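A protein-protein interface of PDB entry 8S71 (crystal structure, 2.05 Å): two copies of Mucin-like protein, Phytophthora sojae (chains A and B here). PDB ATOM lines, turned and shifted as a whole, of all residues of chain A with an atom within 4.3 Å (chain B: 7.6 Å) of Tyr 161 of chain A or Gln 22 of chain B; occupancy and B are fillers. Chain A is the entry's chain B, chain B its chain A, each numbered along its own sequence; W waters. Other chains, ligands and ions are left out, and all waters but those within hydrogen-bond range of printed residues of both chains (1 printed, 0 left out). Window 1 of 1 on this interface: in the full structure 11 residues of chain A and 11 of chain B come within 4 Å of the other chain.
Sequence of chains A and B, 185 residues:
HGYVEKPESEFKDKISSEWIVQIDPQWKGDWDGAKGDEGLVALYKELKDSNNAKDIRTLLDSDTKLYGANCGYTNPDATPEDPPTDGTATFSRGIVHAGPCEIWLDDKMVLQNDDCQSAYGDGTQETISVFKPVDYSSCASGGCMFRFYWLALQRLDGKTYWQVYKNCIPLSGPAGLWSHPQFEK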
ATOM      1  N   ILE A  23      34.031 -30.638  30.445  1.00  0.00           N
ATOM      2  CA  ILE A  23      33.142 -30.903  31.567  1.00  0.00           C
ATOM      3  C   ILE A  23      33.482 -29.975  32.741  1.00  0.00           C
ATOM      4  O   ILE A  23      34.519 -29.313  32.743  1.00  0.00           O
ATOM      5  CB  ILE A  23      33.284 -32.376  31.968  1.00  0.00           C
ATOM      6  CG1 ILE A  23      34.689 -32.668  32.508  1.00  0.00           C
ATOM      7  CG2 ILE A  23      32.935 -33.277  30.789  1.00  0.00           C
ATOM      8  CD1 ILE A  23      34.808 -33.988  33.156  1.00  0.00           C
ATOM      9  N   ASP A  24      32.573 -29.901  33.720  1.00  0.00           N
ATOM     10  CA  ASP A  24      32.851 -29.224  34.977  1.00  0.00           C
ATOM     11  C   ASP A  24      33.995 -29.954  35.686  1.00  0.00           C
ATOM     12  O   ASP A  24      34.156 -31.153  35.572  1.00  0.00           O
ATOM     13  CB  ASP A  24      31.616 -29.142  35.888  1.00  0.00           C
ATOM     14  CG  ASP A  24      30.421 -28.377  35.326  1.00  0.00           C
ATOM     15  OD1 ASP A  24      30.622 -27.292  34.759  1.00  0.00           O
ATOM     16  OD2 ASP A  24      29.287 -28.875  35.461  1.00  0.00           O
ATOM     17  N   PRO A  25      34.848 -29.262  36.450  1.00  0.00           N
ATOM     18  CA  PRO A  25      35.841 -29.946  37.282  1.00  0.00           C
ATOM     19  C   PRO A  25      35.124 -30.976  38.158  1.00  0.00           C
ATOM     20  O   PRO A  25      34.079 -30.680  38.723  1.00  0.00           O
ATOM     21  CB  PRO A  25      36.464 -28.810  38.098  1.00  0.00           C
ATOM     22  CG  PRO A  25      36.218 -27.583  37.271  1.00  0.00           C
ATOM     23  CD  PRO A  25      34.887 -27.798  36.582  1.00  0.00           C
ATOM     24  N   ALA A 152      43.296 -30.343  30.212  1.00  0.00           N
ATOM     25  CA  ALA A 152      43.537 -28.919  30.064  1.00  0.00           C
ATOM     26  C   ALA A 152      42.559 -28.172  30.980  1.00  0.00           C
ATOM     27  O   ALA A 152      41.423 -28.592  31.166  1.00  0.00           O
ATOM     28  CB  ALA A 152      43.419 -28.524  28.607  1.00  0.00           C
ATOM     29  N   LEU A 153      43.044 -27.112  31.614  1.00  0.00           N
ATOM     30  CA  LEU A 153      42.294 -26.349  32.589  1.00  0.00           C
ATOM     31  C   LEU A 153      41.988 -24.985  31.985  1.00  0.00           C
ATOM     32  O   LEU A 153      42.904 -24.207  31.710  1.00  0.00           O
ATOM     33  CB  LEU A 153      43.161 -26.212  33.839  1.00  0.00           C
ATOM     34  CG  LEU A 153      43.729 -27.504  34.417  1.00  0.00           C
ATOM     35  CD1 LEU A 153      44.730 -27.212  35.541  1.00  0.00           C
ATOM     36  CD2 LEU A 153      42.618 -28.410  34.913  1.00  0.00           C
ATOM     37  N   GLN A 154      40.700 -24.730  31.747  1.00  0.00           N
ATOM     38  CA  GLN A 154      40.255 -23.659  30.869  1.00  0.00           C
ATOM     39  C   GLN A 154      39.285 -22.739  31.606  1.00  0.00           C
ATOM     40  O   GLN A 154      38.621 -23.164  32.552  1.00  0.00           O
ATOM     41  CB  GLN A 154      39.551 -24.283  29.668  1.00  0.00           C
ATOM     42  CG  GLN A 154      40.483 -25.079  28.773  1.00  0.00           C
ATOM     43  CD  GLN A 154      41.046 -24.242  27.653  1.00  0.00           C
ATOM     44  OE1 GLN A 154      41.138 -23.021  27.724  1.00  0.00           O
ATOM     45  NE2 GLN A 154      41.440 -24.916  26.589  1.00  0.00           N
ATOM     46  N   LEU A 156      36.031 -19.864  30.808  1.00  0.00           N
ATOM     47  CA  LEU A 156      35.121 -19.126  29.935  1.00  0.00           C
ATOM     48  C   LEU A 156      34.256 -18.254  30.827  1.00  0.00           C
ATOM     49  O   LEU A 156      33.453 -18.793  31.591  1.00  0.00           O
ATOM     50  CB  LEU A 156      34.271 -20.099  29.110  1.00  0.00           C
ATOM     51  CG  LEU A 156      33.133 -19.496  28.297  1.00  0.00           C
ATOM     52  CD1 LEU A 156      33.663 -18.518  27.256  1.00  0.00           C
ATOM     53  CD2 LEU A 156      32.314 -20.595  27.649  1.00  0.00           C
ATOM     54  N   LYS A 159      34.325 -19.015  34.519  1.00  0.00           N
ATOM     55  CA  LYS A 159      33.975 -20.369  34.887  1.00  0.00           C
ATOM     56  C   LYS A 159      35.063 -21.312  34.357  1.00  0.00           C
ATOM     57  O   LYS A 159      35.426 -21.241  33.185  1.00  0.00           O
ATOM     58  CB  LYS A 159      32.578 -20.718  34.380  1.00  0.00           C
ATOM     59  CG  LYS A 159      31.922 -21.793  35.228  1.00  0.00           C
ATOM     60  CD  LYS A 159      30.948 -22.692  34.507  1.00  0.00           C
ATOM     61  CE  LYS A 159      29.988 -23.371  35.465  1.00  0.00           C
ATOM     62  NZ  LYS A 159      28.964 -22.422  35.967  1.00  0.00           N
ATOM     63  N   THR A 160      35.557 -22.198  35.237  1.00  0.00           N
ATOM     64  CA  THR A 160      36.603 -23.163  34.926  1.00  0.00           C
ATOM     65  C   THR A 160      35.990 -24.447  34.345  1.00  0.00           C
ATOM     66  O   THR A 160      34.945 -24.928  34.790  1.00  0.00           O
ATOM     67  CB  THR A 160      37.472 -23.427  36.167  1.00  0.00           C
ATOM     68  OG1 THR A 160      37.787 -22.173  36.779  1.00  0.00           O
ATOM     69  CG2 THR A 160      38.760 -24.155  35.854  1.00  0.00           C
ATOM     70  N   TYR A 161      36.684 -25.031  33.366  1.00  0.00           N
ATOM     71  CA  TYR A 161      36.318 -26.332  32.838  1.00  0.00           C
ATOM     72  C   TYR A 161      37.572 -27.206  32.724  1.00  0.00           C
ATOM     73  O   TYR A 161      38.712 -26.728  32.670  1.00  0.00           O
ATOM     74  CB  TYR A 161      35.603 -26.217  31.484  1.00  0.00           C
ATOM     75  CG  TYR A 161      34.257 -25.495  31.485  1.00  0.00           C
ATOM     76  CD1 TYR A 161      34.182 -24.104  31.442  1.00  0.00           C
ATOM     77  CD2 TYR A 161      33.055 -26.202  31.542  1.00  0.00           C
ATOM     78  CE1 TYR A 161      32.966 -23.437  31.426  1.00  0.00           C
ATOM     79  CE2 TYR A 161      31.830 -25.545  31.563  1.00  0.00           C
ATOM     80  CZ  TYR A 161      31.789 -24.161  31.491  1.00  0.00           C
ATOM     81  OH  TYR A 161      30.596 -23.502  31.496  1.00  0.00           O
ATOM     82  N   TRP A 162      37.334 -28.518  32.704  1.00  0.00           N
ATOM     83  CA  TRP A 162      38.319 -29.496  32.291  1.00  0.00           C
ATOM     84  C   TRP A 162      38.052 -29.961  30.863  1.00  0.00           C
ATOM     85  O   TRP A 162      36.942 -30.399  30.558  1.00  0.00           O
ATOM     86  CB  TRP A 162      38.168 -30.689  33.226  1.00  0.00           C
ATOM     87  CG  TRP A 162      38.705 -30.506  34.611  1.00  0.00           C
ATOM     88  CD1 TRP A 162      39.264 -29.409  35.201  1.00  0.00           C
ATOM     89  CD2 TRP A 162      38.710 -31.558  35.590  1.00  0.00           C
ATOM     90  NE1 TRP A 162      39.644 -29.717  36.488  1.00  0.00           N
ATOM     91  CE2 TRP A 162      39.301 -31.023  36.762  1.00  0.00           C
ATOM     92  CE3 TRP A 162      38.292 -32.898  35.586  1.00  0.00           C
ATOM     93  CZ2 TRP A 162      39.479 -31.800  37.915  1.00  0.00           C
ATOM     94  CZ3 TRP A 162      38.460 -33.655  36.729  1.00  0.00           C
ATOM     95  CH2 TRP A 162      39.064 -33.118  37.874  1.00  0.00           C
ATOM     96  N   GLN A 163      39.068 -29.882  30.004  1.00  0.00           N
ATOM     97  CA  GLN A 163      39.037 -30.497  28.699  1.00  0.00           C
ATOM     98  C   GLN A 163      39.935 -31.721  28.763  1.00  0.00           C
ATOM     99  O   GLN A 163      41.090 -31.640  29.208  1.00  0.00           O
ATOM    100  CB  GLN A 163      39.558 -29.529  27.637  1.00  0.00           C
ATOM    101  CG  GLN A 163      38.645 -28.372  27.319  1.00  0.00           C
ATOM    102  CD  GLN A 163      39.295 -27.412  26.347  1.00  0.00           C
ATOM    103  OE1 GLN A 163      40.500 -27.455  26.087  1.00  0.00           O
ATOM    104  NE2 GLN A 163      38.503 -26.485  25.853  1.00  0.00           N
ATOM    105  N   HIS B   1      27.732 -11.357  31.816  1.00  0.00           N
ATOM    106  CA  HIS B   1      27.180 -11.440  33.192  1.00  0.00           C
ATOM    107  C   HIS B   1      26.508 -10.122  33.543  1.00  0.00           C
ATOM    108  O   HIS B   1      26.824  -9.075  32.960  1.00  0.00           O
ATOM    109  CB  HIS B   1      28.260 -11.824  34.210  1.00  0.00           C
ATOM    110  CG  HIS B   1      28.641 -13.269  34.122  1.00  0.00           C
ATOM    111  ND1 HIS B   1      29.179 -13.844  32.984  1.00  0.00           N
ATOM    112  CD2 HIS B   1      28.563 -14.256  35.046  1.00  0.00           C
ATOM    113  CE1 HIS B   1      29.373 -15.135  33.221  1.00  0.00           C
ATOM    114  NE2 HIS B   1      29.029 -15.398  34.473  1.00  0.00           N
ATOM    115  N   GLU B  18      24.864 -14.740  36.660  1.00  0.00           N
ATOM    116  CA  GLU B  18      25.163 -15.726  35.632  1.00  0.00           C
ATOM    117  C   GLU B  18      24.007 -15.876  34.641  1.00  0.00           C
ATOM    118  O   GLU B  18      22.846 -15.572  34.957  1.00  0.00           O
ATOM    119  CB  GLU B  18      25.364 -17.073  36.309  1.00  0.00           C
ATOM    120  CG  GLU B  18      25.999 -18.129  35.428  1.00  0.00           C
ATOM    121  CD  GLU B  18      26.522 -19.316  36.224  1.00  0.00           C
ATOM    122  OE1 GLU B  18      25.706 -20.188  36.599  1.00  0.00           O
ATOM    123  OE2 GLU B  18      27.725 -19.339  36.498  1.00  0.00           O
ATOM    124  N   TRP B  19      24.367 -16.386  33.460  1.00  0.00           N
ATOM    125  CA  TRP B  19      23.435 -16.900  32.459  1.00  0.00           C
ATOM    126  C   TRP B  19      22.582 -18.036  33.036  1.00  0.00           C
ATOM    127  O   TRP B  19      22.956 -18.663  34.033  1.00  0.00           O
ATOM    128  CB  TRP B  19      24.229 -17.335  31.216  1.00  0.00           C
ATOM    129  CG  TRP B  19      25.490 -18.091  31.522  1.00  0.00           C
ATOM    130  CD1 TRP B  19      26.747 -17.567  31.517  1.00  0.00           C
ATOM    131  CD2 TRP B  19      25.634 -19.476  31.907  1.00  0.00           C
ATOM    132  NE1 TRP B  19      27.665 -18.532  31.840  1.00  0.00           N
ATOM    133  CE2 TRP B  19      27.015 -19.708  32.100  1.00  0.00           C
ATOM    134  CE3 TRP B  19      24.747 -20.542  32.116  1.00  0.00           C
ATOM    135  CZ2 TRP B  19      27.522 -20.952  32.474  1.00  0.00           C
ATOM    136  CZ3 TRP B  19      25.247 -21.758  32.523  1.00  0.00           C
ATOM    137  CH2 TRP B  19      26.616 -21.963  32.708  1.00  0.00           C
ATOM    138  N   ILE B  20      21.399 -18.258  32.440  1.00  0.00           N
ATOM    139  CA  ILE B  20      20.503 -19.302  32.906  1.00  0.00           C
ATOM    140  C   ILE B  20      20.899 -20.617  32.231  1.00  0.00           C
ATOM    141  O   ILE B  20      20.907 -21.665  32.873  1.00  0.00           O
ATOM    142  CB  ILE B  20      18.997 -18.960  32.747  1.00  0.00           C
ATOM    143  CG1 ILE B  20      18.109 -20.048  33.357  1.00  0.00           C
ATOM    144  CG2 ILE B  20      18.612 -18.734  31.298  1.00  0.00           C
ATOM    145  CD1 ILE B  20      18.313 -20.253  34.851  1.00  0.00           C
ATOM    146  N   VAL B  21      21.315 -20.554  30.965  1.00  0.00           N
ATOM    147  CA  VAL B  21      21.971 -21.682  30.309  1.00  0.00           C
ATOM    148  C   VAL B  21      23.105 -21.191  29.420  1.00  0.00           C
ATOM    149  O   VAL B  21      23.188 -20.013  29.084  1.00  0.00           O
ATOM    150  CB  VAL B  21      20.969 -22.486  29.464  1.00  0.00           C
ATOM    151  CG1 VAL B  21      19.888 -23.121  30.325  1.00  0.00           C
ATOM    152  CG2 VAL B  21      20.361 -21.619  28.372  1.00  0.00           C
ATOM    153  N   GLN B  22      23.946 -22.148  29.019  1.00  0.00           N
ATOM    154  CA  GLN B  22      25.041 -21.943  28.089  1.00  0.00           C
ATOM    155  C   GLN B  22      25.128 -23.184  27.208  1.00  0.00           C
ATOM    156  O   GLN B  22      25.478 -24.251  27.694  1.00  0.00           O
ATOM    157  CB  GLN B  22      26.324 -21.690  28.879  1.00  0.00           C
ATOM    158  CG  GLN B  22      27.582 -21.557  28.029  1.00  0.00           C
ATOM    159  CD  GLN B  22      28.742 -21.146  28.910  1.00  0.00           C
ATOM    160  OE1 GLN B  22      29.386 -20.122  28.697  1.00  0.00           O
ATOM    161  NE2 GLN B  22      28.990 -21.938  29.943  1.00  0.00           N
ATOM    162  N   ILE B  23      24.795 -23.027  25.921  1.00  0.00           N
ATOM    163  CA  ILE B  23      24.499 -24.140  25.039  1.00  0.00           C
ATOM    164  C   ILE B  23      25.197 -23.951  23.690  1.00  0.00           C
ATOM    165  O   ILE B  23      25.744 -22.883  23.386  1.00  0.00           O
ATOM    166  CB  ILE B  23      22.975 -24.213  24.877  1.00  0.00           C
ATOM    167  CG1 ILE B  23      22.406 -22.911  24.299  1.00  0.00           C
ATOM    168  CG2 ILE B  23      22.338 -24.589  26.209  1.00  0.00           C
ATOM    169  CD1 ILE B  23      20.949 -22.979  23.882  1.00  0.00           C
ATOM    170  N   ASP B  24      25.140 -24.982  22.852  1.00  0.00           N
ATOM    171  CA  ASP B  24      25.620 -24.847  21.486  1.00  0.00           C
ATOM    172  C   ASP B  24      24.679 -23.910  20.739  1.00  0.00           C
ATOM    173  O   ASP B  24      23.492 -23.851  21.034  1.00  0.00           O
ATOM    174  CB  ASP B  24      25.717 -26.197  20.771  1.00  0.00           C
ATOM    175  CG  ASP B  24      26.582 -27.212  21.502  1.00  0.00           C
ATOM    176  OD1 ASP B  24      27.810 -26.989  21.600  1.00  0.00           O
ATOM    177  OD2 ASP B  24      26.007 -28.212  21.999  1.00  0.00           O
ATOM    178  N   PRO B  25      25.136 -23.184  19.706  1.00  0.00           N
ATOM    179  CA  PRO B  25      24.211 -22.402  18.896  1.00  0.00           C
ATOM    180  C   PRO B  25      23.147 -23.335  18.347  1.00  0.00           C
ATOM    181  O   PRO B  25      23.460 -24.460  17.970  1.00  0.00           O
ATOM    182  CB  PRO B  25      25.086 -21.805  17.799  1.00  0.00           C
ATOM    183  CG  PRO B  25      26.473 -21.861  18.395  1.00  0.00           C
ATOM    184  CD  PRO B  25      26.509 -23.148  19.196  1.00  0.00           C
ATOM    185  N   LEU B  66      15.709 -26.052  26.965  1.00  0.00           N
ATOM    186  CA  LEU B  66      16.874 -25.774  26.145  1.00  0.00           C
ATOM    187  C   LEU B  66      17.388 -24.352  26.392  1.00  0.00           C
ATOM    188  O   LEU B  66      18.578 -24.106  26.315  1.00  0.00           O
ATOM    189  CB  LEU B  66      16.432 -25.957  24.693  1.00  0.00           C
ATOM    190  CG  LEU B  66      17.379 -25.477  23.603  1.00  0.00           C
ATOM    191  CD1 LEU B  66      18.712 -26.211  23.680  1.00  0.00           C
ATOM    192  CD2 LEU B  66      16.729 -25.701  22.242  1.00  0.00           C
ATOM    193  N   TYR B  67      16.476 -23.404  26.625  1.00  0.00           N
ATOM    194  CA  TYR B  67      16.815 -21.988  26.687  1.00  0.00           C
ATOM    195  C   TYR B  67      16.722 -21.462  28.113  1.00  0.00           C
ATOM    196  O   TYR B  67      16.919 -20.270  28.312  1.00  0.00           O
ATOM    197  CB  TYR B  67      15.941 -21.187  25.724  1.00  0.00           C
ATOM    198  CG  TYR B  67      16.243 -21.503  24.275  1.00  0.00           C
ATOM    199  CD1 TYR B  67      17.496 -21.245  23.721  1.00  0.00           C
ATOM    200  CD2 TYR B  67      15.295 -22.102  23.460  1.00  0.00           C
ATOM    201  CE1 TYR B  67      17.776 -21.548  22.398  1.00  0.00           C
ATOM    202  CE2 TYR B  67      15.557 -22.395  22.133  1.00  0.00           C
ATOM    203  CZ  TYR B  67      16.795 -22.106  21.596  1.00  0.00           C
ATOM    204  OH  TYR B  67      17.034 -22.404  20.284  1.00  0.00           O
ATOM    205  N   GLY B  68      16.407 -22.339  29.078  1.00  0.00           N
ATOM    206  CA  GLY B  68      16.417 -21.986  30.491  1.00  0.00           C
ATOM    207  C   GLY B  68      15.051 -21.556  31.042  1.00  0.00           C
ATOM    208  O   GLY B  68      14.137 -21.160  30.309  1.00  0.00           O
ATOM    209  N   ALA B 152      24.202 -13.841  24.547  1.00  0.00           N
ATOM    210  CA  ALA B 152      25.608 -13.511  24.409  1.00  0.00           C
ATOM    211  C   ALA B 152      26.247 -14.595  23.542  1.00  0.00           C
ATOM    212  O   ALA B 152      25.957 -15.769  23.709  1.00  0.00           O
ATOM    213  CB  ALA B 152      26.287 -13.376  25.764  1.00  0.00           C
ATOM    214  N   GLN B 154      29.608 -16.302  22.477  1.00  0.00           N
ATOM    215  CA  GLN B 154      30.831 -16.491  23.233  1.00  0.00           C
ATOM    216  C   GLN B 154      31.735 -17.506  22.540  1.00  0.00           C
ATOM    217  O   GLN B 154      31.260 -18.325  21.752  1.00  0.00           O
ATOM    218  CB  GLN B 154      30.429 -16.959  24.625  1.00  0.00           C
ATOM    219  CG  GLN B 154      29.857 -15.840  25.469  1.00  0.00           C
ATOM    220  CD  GLN B 154      30.906 -15.076  26.237  1.00  0.00           C
ATOM    221  OE1 GLN B 154      30.641 -14.603  27.332  1.00  0.00           O
ATOM    222  NE2 GLN B 154      32.120 -15.000  25.728  1.00  0.00           N
ATOM    223  N   ARG B 155      33.034 -17.451  22.842  1.00  0.00           N
ATOM    224  CA  ARG B 155      33.983 -18.404  22.285  1.00  0.00           C
ATOM    225  C   ARG B 155      34.858 -18.969  23.403  1.00  0.00           C
ATOM    226  O   ARG B 155      35.427 -18.223  24.197  1.00  0.00           O
ATOM    227  CB  ARG B 155      34.890 -17.756  21.235  1.00  0.00           C
ATOM    228  CG  ARG B 155      34.231 -17.430  19.899  1.00  0.00           C
ATOM    229  CD  ARG B 155      34.314 -18.575  18.917  1.00  0.00           C
ATOM    230  NE  ARG B 155      33.819 -18.260  17.577  1.00  0.00           N
ATOM    231  CZ  ARG B 155      34.406 -17.423  16.715  1.00  0.00           C
ATOM    232  NH1 ARG B 155      35.467 -16.729  17.087  1.00  0.00           N
ATOM    233  NH2 ARG B 155      33.933 -17.274  15.486  1.00  0.00           N
ATOM    234  N   LEU B 156      35.014 -20.301  23.399  1.00  0.00           N
ATOM    235  CA  LEU B 156      35.996 -20.984  24.226  1.00  0.00           C
ATOM    236  C   LEU B 156      36.855 -21.849  23.310  1.00  0.00           C
ATOM    237  O   LEU B 156      36.369 -22.816  22.710  1.00  0.00           O
ATOM    238  CB  LEU B 156      35.269 -21.795  25.308  1.00  0.00           C
ATOM    239  CG  LEU B 156      36.148 -22.661  26.207  1.00  0.00           C
ATOM    240  CD1 LEU B 156      37.194 -21.841  26.950  1.00  0.00           C
ATOM    241  CD2 LEU B 156      35.274 -23.440  27.176  1.00  0.00           C
ATOM    242  N   TYR B 161      29.631 -20.558  21.688  1.00  0.00           N
ATOM    243  CA  TYR B 161      28.507 -20.896  22.549  1.00  0.00           C
ATOM    244  C   TYR B 161      27.524 -19.725  22.577  1.00  0.00           C
ATOM    245  O   TYR B 161      27.886 -18.562  22.427  1.00  0.00           O
ATOM    246  CB  TYR B 161      28.954 -21.259  23.976  1.00  0.00           C
ATOM    247  CG  TYR B 161      29.795 -22.531  24.034  1.00  0.00           C
ATOM    248  CD1 TYR B 161      29.190 -23.784  24.054  1.00  0.00           C
ATOM    249  CD2 TYR B 161      31.182 -22.486  23.921  1.00  0.00           C
ATOM    250  CE1 TYR B 161      29.941 -24.950  24.027  1.00  0.00           C
ATOM    251  CE2 TYR B 161      31.943 -23.645  23.895  1.00  0.00           C
ATOM    252  CZ  TYR B 161      31.322 -24.877  23.957  1.00  0.00           C
ATOM    253  OH  TYR B 161      32.070 -26.022  23.944  1.00  0.00           O
ATOM    254  N   TRP B 162      26.261 -20.078  22.782  1.00  0.00           N
ATOM    255  CA  TRP B 162      25.222 -19.154  23.176  1.00  0.00           C
ATOM    256  C   TRP B 162      25.047 -19.198  24.685  1.00  0.00           C
ATOM    257  O   TRP B 162      24.857 -20.292  25.254  1.00  0.00           O
ATOM    258  CB  TRP B 162      23.911 -19.568  22.516  1.00  0.00           C
ATOM    259  CG  TRP B 162      23.816 -19.253  21.054  1.00  0.00           C
ATOM    260  CD1 TRP B 162      24.768 -18.760  20.211  1.00  0.00           C
ATOM    261  CD2 TRP B 162      22.613 -19.399  20.274  1.00  0.00           C
ATOM    262  NE1 TRP B 162      24.251 -18.632  18.945  1.00  0.00           N
ATOM    263  CE2 TRP B 162      22.928 -19.010  18.957  1.00  0.00           C
ATOM    264  CE3 TRP B 162      21.318 -19.835  20.565  1.00  0.00           C
ATOM    265  CZ2 TRP B 162      21.978 -19.037  17.941  1.00  0.00           C
ATOM    266  CZ3 TRP B 162      20.380 -19.860  19.552  1.00  0.00           C
ATOM    267  CH2 TRP B 162      20.706 -19.458  18.261  1.00  0.00           C
ATOM    268  N   GLN B 163      25.086 -18.004  25.301  1.00  0.00           N
ATOM    269  CA  GLN B 163      24.710 -17.844  26.700  1.00  0.00           C
ATOM    270  C   GLN B 163      23.376 -17.104  26.741  1.00  0.00           C
ATOM    271  O   GLN B 163      23.218 -16.059  26.100  1.00  0.00           O
ATOM    272  CB  GLN B 163      25.767 -17.065  27.494  1.00  0.00           C
ATOM    273  CG  GLN B 163      27.104 -17.760  27.707  1.00  0.00           C
ATOM    274  CD  GLN B 163      28.062 -16.877  28.483  1.00  0.00           C
ATOM    275  OE1 GLN B 163      27.865 -15.676  28.621  1.00  0.00           O
ATOM    276  NE2 GLN B 163      29.139 -17.452  28.979  1.00  0.00           N
ATOM    277  N   VAL B 164      22.441 -17.629  27.533  1.00  0.00           N
ATOM    278  CA  VAL B 164      21.136 -17.013  27.651  1.00  0.00           C
ATOM    279  C   VAL B 164      20.993 -16.371  29.016  1.00  0.00           C
ATOM    280  O   VAL B 164      21.120 -17.023  30.057  1.00  0.00           O
ATOM    281  CB  VAL B 164      19.992 -17.998  27.364  1.00  0.00           C
ATOM    282  CG1 VAL B 164      18.634 -17.327  27.492  1.00  0.00           C
ATOM    283  CG2 VAL B 164      20.170 -18.621  25.998  1.00  0.00           C
ATOM    284  N   TYR B 165      20.651 -15.080  28.970  1.00  0.00           N
ATOM    285  CA  TYR B 165      20.348 -14.335  30.170  1.00  0.00           C
ATOM    286  C   TYR B 165      18.875 -13.953  30.104  1.00  0.00           C
ATOM    287  O   TYR B 165      18.423 -13.444  29.083  1.00  0.00           O
ATOM    288  CB  TYR B 165      21.242 -13.098  30.292  1.00  0.00           C
ATOM    289  CG  TYR B 165      22.733 -13.379  30.343  1.00  0.00           C
ATOM    290  CD1 TYR B 165      23.437 -13.725  29.202  1.00  0.00           C
ATOM    291  CD2 TYR B 165      23.428 -13.325  31.543  1.00  0.00           C
ATOM    292  CE1 TYR B 165      24.798 -13.971  29.249  1.00  0.00           C
ATOM    293  CE2 TYR B 165      24.771 -13.637  31.614  1.00  0.00           C
ATOM    294  CZ  TYR B 165      25.463 -13.941  30.463  1.00  0.00           C
ATOM    295  OH  TYR B 165      26.795 -14.242  30.509  1.00  0.00           O
HETATM  296  O   HOH W   1      30.454 -18.375  32.424  1.00  0.00           O
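The side-chain amide oxygen (OE1) of Gln 22 of chain B lies within hydrogen-bond range of the side-chain amide nitrogen (NE2) of Gln 163 of chain B (2.7 Å).
N of Tyr 161 of chain A lies within hydrogen-bond range of O of Gln 154 of chain A (2.8 Å).
Of the printed residues of chain B, Tyr 161 of chain A touches Gln 22 (2.7 Å).
Printed residues of chain A within 4 Å of Gln 22 of chain B: Leu 156 (3.1 Å) and Tyr 161 (2.7 Å).
Of the printed residues of chain A, Arg 155 of chain B touches Leu 156.
Of the printed residues of chain A, Glu 18 of chain B touches Lys 159.
Printed residues of chain B within 4 Å of Lys 159 of chain A: Glu 18 (3.4 Å).
Printed residues of chain B within 4 Å of Leu 156 of chain A: Gln 22, Arg 155 and Leu 156.
Of the printed residues of chain A, Leu 156 of chain B touches Leu 156.
His 1 of chain B touches none of the printed residues of chain A.
Tyr 67 of chain B touches none of the printed residues of chain A.
The nearest printed residue of chain B that does not touch Tyr 161 of chain A is Trp 19 of chain B (4.1 Å).
The nearest printed residue of chain B that does not touch Lys 159 of chain A is Trp 19 of chain B (4.04 Å).
Leu 156 of chain A touches its own counterpart, Leu 156 of chain B.
9 positions are printed for both chains.
Hydrophobic or aromatic side chains of chain A within 4 Å of the printed part of chain B: Leu 156 and Tyr 161.
Of the 21 printed residues of chain B, 4 touch a printed residue of chain A.
Along chain B the printed residues that touch a printed residue of chain A span positions 18 to 156.
Among the printed residues, 5 pairs touch across the chains.
Water W1 lies within hydrogen-bond range of the indole nitrogen of Trp 19 of chain B (2.9 Å) and the backbone carbonyl oxygen of Leu 156 of chain A (3.1 Å).
The side-chain carboxylate of Glu 18 of chain B is in salt-bridge range of the side-chain amino group of Lys 159 of chain A (3.4 Å).
The side-chain hydroxyl of Tyr 161 of chain A lies within hydrogen-bond range of the side-chain amide nitrogen of Gln 22 of chain B (2.7 Å).
Among the printed residues, pairs that only touch across the chains: Leu 156 of chain A with Gln 22 of chain B, Leu 156 of chain A with Arg 155 of chain B and Leu 156 of chain A with Leu 156 of chain B.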
